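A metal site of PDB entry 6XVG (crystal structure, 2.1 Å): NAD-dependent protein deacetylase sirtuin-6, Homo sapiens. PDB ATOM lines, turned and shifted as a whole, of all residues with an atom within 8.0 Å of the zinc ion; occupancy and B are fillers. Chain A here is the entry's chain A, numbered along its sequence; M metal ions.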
ATOM      1  N   GLU A 138      -2.304  27.371  -5.994  1.00  0.00           N
ATOM      2  CA  GLU A 138      -2.302  26.163  -5.114  1.00  0.00           C
ATOM      3  C   GLU A 138      -1.207  25.200  -5.602  1.00  0.00           C
ATOM      4  O   GLU A 138      -1.074  25.009  -6.823  1.00  0.00           O
ATOM      5  CB  GLU A 138      -3.684  25.522  -5.141  1.00  0.00           C
ATOM      6  CG  GLU A 138      -3.800  24.309  -4.231  1.00  0.00           C
ATOM      7  CD  GLU A 138      -5.200  23.730  -4.132  1.00  0.00           C
ATOM      8  OE1 GLU A 138      -6.118  24.512  -3.879  1.00  0.00           O
ATOM      9  OE2 GLU A 138      -5.378  22.502  -4.327  1.00  0.00           O
ATOM     10  N   CYS A 139      -0.466  24.619  -4.663  1.00  0.00           N
ATOM     11  CA  CYS A 139       0.567  23.586  -4.947  1.00  0.00           C
ATOM     12  C   CYS A 139      -0.134  22.271  -5.312  1.00  0.00           C
ATOM     13  O   CYS A 139      -0.911  21.744  -4.471  1.00  0.00           O
ATOM     14  CB  CYS A 139       1.474  23.375  -3.731  1.00  0.00           C
ATOM     15  SG  CYS A 139       2.771  22.142  -3.992  1.00  0.00           S
ATOM     16  N   ALA A 140       0.150  21.751  -6.505  1.00  0.00           N
ATOM     17  CA  ALA A 140      -0.329  20.436  -6.999  1.00  0.00           C
ATOM     18  C   ALA A 140       0.037  19.315  -6.007  1.00  0.00           C
ATOM     19  O   ALA A 140      -0.789  18.418  -5.795  1.00  0.00           O
ATOM     20  CB  ALA A 140       0.247  20.165  -8.366  1.00  0.00           C
ATOM     21  N   LYS A 141       1.213  19.388  -5.381  1.00  0.00           N
ATOM     22  CA  LYS A 141       1.763  18.335  -4.493  1.00  0.00           C
ATOM     23  C   LYS A 141       1.102  18.422  -3.107  1.00  0.00           C
ATOM     24  O   LYS A 141       0.445  17.446  -2.728  1.00  0.00           O
ATOM     25  CB  LYS A 141       3.297  18.432  -4.434  1.00  0.00           C
ATOM     26  CG  LYS A 141       3.984  17.411  -3.540  1.00  0.00           C
ATOM     27  CD  LYS A 141       5.504  17.488  -3.558  1.00  0.00           C
ATOM     28  CE  LYS A 141       6.134  17.030  -4.857  1.00  0.00           C
ATOM     29  NZ  LYS A 141       7.579  16.747  -4.706  1.00  0.00           N
ATOM     30  N   CYS A 142       1.263  19.512  -2.360  1.00  0.00           N
ATOM     31  CA  CYS A 142       0.875  19.575  -0.912  1.00  0.00           C
ATOM     32  C   CYS A 142      -0.417  20.388  -0.693  1.00  0.00           C
ATOM     33  O   CYS A 142      -0.879  20.431   0.469  1.00  0.00           O
ATOM     34  CB  CYS A 142       2.010  20.105  -0.044  1.00  0.00           C
ATOM     35  SG  CYS A 142       2.418  21.861  -0.274  1.00  0.00           S
ATOM     36  N   LYS A 143      -0.989  21.005  -1.731  1.00  0.00           N
ATOM     37  CA  LYS A 143      -2.305  21.724  -1.691  1.00  0.00           C
ATOM     38  C   LYS A 143      -2.217  23.050  -0.915  1.00  0.00           C
ATOM     39  O   LYS A 143      -3.263  23.695  -0.716  1.00  0.00           O
ATOM     40  CB  LYS A 143      -3.388  20.818  -1.104  1.00  0.00           C
ATOM     41  CG  LYS A 143      -3.604  19.557  -1.938  1.00  0.00           C
ATOM     42  CD  LYS A 143      -4.784  18.707  -1.542  1.00  0.00           C
ATOM     43  CE  LYS A 143      -4.851  17.422  -2.345  1.00  0.00           C
ATOM     44  NZ  LYS A 143      -5.298  16.260  -1.536  1.00  0.00           N
ATOM     45  N   THR A 144      -1.024  23.499  -0.507  1.00  0.00           N
ATOM     46  CA  THR A 144      -0.807  24.830   0.127  1.00  0.00           C
ATOM     47  C   THR A 144      -1.210  25.936  -0.851  1.00  0.00           C
ATOM     48  O   THR A 144      -0.798  25.885  -2.019  1.00  0.00           O
ATOM     49  CB  THR A 144       0.649  25.028   0.574  1.00  0.00           C
ATOM     50  OG1 THR A 144       0.936  24.025   1.548  1.00  0.00           O
ATOM     51  CG2 THR A 144       0.918  26.393   1.169  1.00  0.00           C
ATOM     52  N   GLN A 145      -1.955  26.931  -0.374  1.00  0.00           N
ATOM     53  CA  GLN A 145      -2.402  28.099  -1.183  1.00  0.00           C
ATOM     54  C   GLN A 145      -1.518  29.306  -0.860  1.00  0.00           C
ATOM     55  O   GLN A 145      -1.064  29.442   0.259  1.00  0.00           O
ATOM     56  CB  GLN A 145      -3.889  28.365  -0.955  1.00  0.00           C
ATOM     57  CG  GLN A 145      -4.711  27.159  -1.364  1.00  0.00           C
ATOM     58  CD  GLN A 145      -6.176  27.474  -1.466  1.00  0.00           C
ATOM     59  OE1 GLN A 145      -6.716  28.190  -0.650  1.00  0.00           O
ATOM     60  NE2 GLN A 145      -6.828  26.941  -2.493  1.00  0.00           N
ATOM     61  N   TYR A 146      -1.264  30.111  -1.884  1.00  0.00           N
ATOM     62  CA  TYR A 146      -0.536  31.388  -1.820  1.00  0.00           C
ATOM     63  C   TYR A 146      -1.497  32.472  -2.296  1.00  0.00           C
ATOM     64  O   TYR A 146      -2.000  32.388  -3.428  1.00  0.00           O
ATOM     65  CB  TYR A 146       0.720  31.326  -2.670  1.00  0.00           C
ATOM     66  CG  TYR A 146       1.702  30.269  -2.250  1.00  0.00           C
ATOM     67  CD1 TYR A 146       1.464  28.927  -2.486  1.00  0.00           C
ATOM     68  CD2 TYR A 146       2.882  30.609  -1.606  1.00  0.00           C
ATOM     69  CE1 TYR A 146       2.362  27.946  -2.089  1.00  0.00           C
ATOM     70  CE2 TYR A 146       3.798  29.652  -1.202  1.00  0.00           C
ATOM     71  CZ  TYR A 146       3.529  28.315  -1.437  1.00  0.00           C
ATOM     72  OH  TYR A 146       4.432  27.376  -1.034  1.00  0.00           O
ATOM     73  N   LEU A 163       7.078  27.682  -8.098  1.00  0.00           N
ATOM     74  CA  LEU A 163       7.178  26.390  -7.388  1.00  0.00           C
ATOM     75  C   LEU A 163       6.878  26.643  -5.909  1.00  0.00           C
ATOM     76  O   LEU A 163       7.153  27.742  -5.434  1.00  0.00           O
ATOM     77  CB  LEU A 163       8.565  25.765  -7.596  1.00  0.00           C
ATOM     78  CG  LEU A 163       8.921  25.362  -9.031  1.00  0.00           C
ATOM     79  CD1 LEU A 163       7.860  24.437  -9.615  1.00  0.00           C
ATOM     80  CD2 LEU A 163       9.110  26.580  -9.907  1.00  0.00           C
ATOM     81  N   CYS A 164       6.356  25.639  -5.224  1.00  0.00           N
ATOM     82  CA  CYS A 164       6.022  25.681  -3.778  1.00  0.00           C
ATOM     83  C   CYS A 164       7.302  25.929  -2.980  1.00  0.00           C
ATOM     84  O   CYS A 164       8.351  25.417  -3.376  1.00  0.00           O
ATOM     85  CB  CYS A 164       5.386  24.366  -3.371  1.00  0.00           C
ATOM     86  SG  CYS A 164       4.675  24.422  -1.715  1.00  0.00           S
ATOM     87  N   THR A 165       7.205  26.701  -1.892  1.00  0.00           N
ATOM     88  CA  THR A 165       8.358  27.089  -1.039  1.00  0.00           C
ATOM     89  C   THR A 165       8.187  26.543   0.383  1.00  0.00           C
ATOM     90  O   THR A 165       9.012  26.881   1.237  1.00  0.00           O
ATOM     91  CB  THR A 165       8.541  28.617  -0.991  1.00  0.00           C
ATOM     92  OG1 THR A 165       7.377  29.203  -0.413  1.00  0.00           O
ATOM     93  CG2 THR A 165       8.791  29.223  -2.355  1.00  0.00           C
ATOM     94  N   VAL A 166       7.172  25.713   0.632  1.00  0.00           N
ATOM     95  CA  VAL A 166       6.911  25.091   1.958  1.00  0.00           C
ATOM     96  C   VAL A 166       8.091  24.169   2.307  1.00  0.00           C
ATOM     97  O   VAL A 166       8.660  23.537   1.386  1.00  0.00           O
ATOM     98  CB  VAL A 166       5.581  24.331   1.981  1.00  0.00           C
ATOM     99  CG1 VAL A 166       5.362  23.517   3.246  1.00  0.00           C
ATOM    100  CG2 VAL A 166       4.409  25.278   1.751  1.00  0.00           C
ATOM    101  N   ALA A 167       8.418  24.102   3.612  1.00  0.00           N
ATOM    102  CA  ALA A 167       9.347  23.131   4.238  1.00  0.00           C
ATOM    103  C   ALA A 167       8.558  21.858   4.593  1.00  0.00           C
ATOM    104  O   ALA A 167       9.204  20.821   4.825  1.00  0.00           O
ATOM    105  CB  ALA A 167       9.986  23.744   5.459  1.00  0.00           C
ATOM    106  N   CYS A 175       9.424  21.732  -0.724  1.00  0.00           N
ATOM    107  CA  CYS A 175       8.373  20.984  -1.471  1.00  0.00           C
ATOM    108  C   CYS A 175       8.612  21.064  -2.984  1.00  0.00           C
ATOM    109  O   CYS A 175       8.523  20.023  -3.653  1.00  0.00           O
ATOM    110  CB  CYS A 175       6.971  21.507  -1.139  1.00  0.00           C
ATOM    111  SG  CYS A 175       5.690  20.803  -2.207  1.00  0.00           S
ATOM    112  N   ARG A 176       8.837  22.262  -3.517  1.00  0.00           N
ATOM    113  CA  ARG A 176       9.160  22.516  -4.947  1.00  0.00           C
ATOM    114  C   ARG A 176       7.990  22.069  -5.852  1.00  0.00           C
ATOM    115  O   ARG A 176       8.189  22.050  -7.087  1.00  0.00           O
ATOM    116  CB  ARG A 176      10.473  21.801  -5.330  1.00  0.00           C
ATOM    117  CG  ARG A 176      11.751  22.610  -5.194  1.00  0.00           C
ATOM    118  CD  ARG A 176      12.928  21.921  -5.903  1.00  0.00           C
ATOM    119  NE  ARG A 176      12.773  21.673  -7.346  1.00  0.00           N
ATOM    120  CZ  ARG A 176      12.592  20.485  -7.929  1.00  0.00           C
ATOM    121  NH1 ARG A 176      12.555  19.364  -7.228  1.00  0.00           N
ATOM    122  NH2 ARG A 176      12.435  20.414  -9.241  1.00  0.00           N
ATOM    123  N   GLY A 177       6.812  21.745  -5.296  1.00  0.00           N
ATOM    124  CA  GLY A 177       5.601  21.387  -6.066  1.00  0.00           C
ATOM    125  C   GLY A 177       5.211  22.463  -7.061  1.00  0.00           C
ATOM    126  O   GLY A 177       5.568  23.647  -6.866  1.00  0.00           O
ATOM    127  N   GLU A 178       4.503  22.079  -8.131  1.00  0.00           N
ATOM    128  CA  GLU A 178       4.046  22.993  -9.213  1.00  0.00           C
ATOM    129  C   GLU A 178       2.824  23.786  -8.715  1.00  0.00           C
ATOM    130  O   GLU A 178       1.810  23.148  -8.286  1.00  0.00           O
ATOM    131  CB  GLU A 178       3.734  22.192 -10.478  1.00  0.00           C
ATOM    132  N   LEU A 179       2.916  25.118  -8.748  1.00  0.00           N
ATOM    133  CA  LEU A 179       1.809  26.029  -8.353  1.00  0.00           C
ATOM    134  C   LEU A 179       0.886  26.219  -9.555  1.00  0.00           C
ATOM    135  O   LEU A 179       1.385  26.523 -10.661  1.00  0.00           O
ATOM    136  CB  LEU A 179       2.374  27.376  -7.870  1.00  0.00           C
ATOM    137  CG  LEU A 179       3.315  27.363  -6.661  1.00  0.00           C
ATOM    138  CD1 LEU A 179       3.546  28.784  -6.160  1.00  0.00           C
ATOM    139  CD2 LEU A 179       2.779  26.476  -5.524  1.00  0.00           C
HETATM  140 ZN    ZN M   1       3.802  22.285  -1.919  1.00  0.00          ZN
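The zinc ion is bound by SG of Cys 142 (2.2 Å), SG of Cys 164 (2.3 Å), SG of Cys 139 (2.3 Å) and SG of Cys 175 (2.4 Å).
The zinc ion has four donor atoms within binding distance.
SG of Cys 164 sits close to N of Val 166.
The backbone NH of Arg 176 lies within hydrogen-bond range of the backbone carbonyl oxygen of Cys 164 (3.2 Å).
N of Lys 141 lies close to SG of Cys 139, 3.5 Å away.
The backbone NH (N) of Cys 164 lies within hydrogen-bond range of the backbone carbonyl oxygen (O) of Gly 177.
The side-chain sulfur (SG) of Cys 175 lies close to the backbone NH (N) of Gly 177, 3.4 Å away.
The backbone carbonyl oxygen (O) of Thr 144 is in hydrogen-bond range of the backbone NH (N) of Cys 139, 3.0 Å away.
The side-chain sulfur (SG) of Cys 142 lies close to the side-chain hydroxyl (OG1) of Thr 144.
OH of Tyr 146 lies close to SG of Cys 164 (3.0 Å).
Of the 19 residues printed, 4 come within 4 Å of the zinc ion.
The nearest printed residue that does not touch the zinc ion is Gly 177 (4.6 Å).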
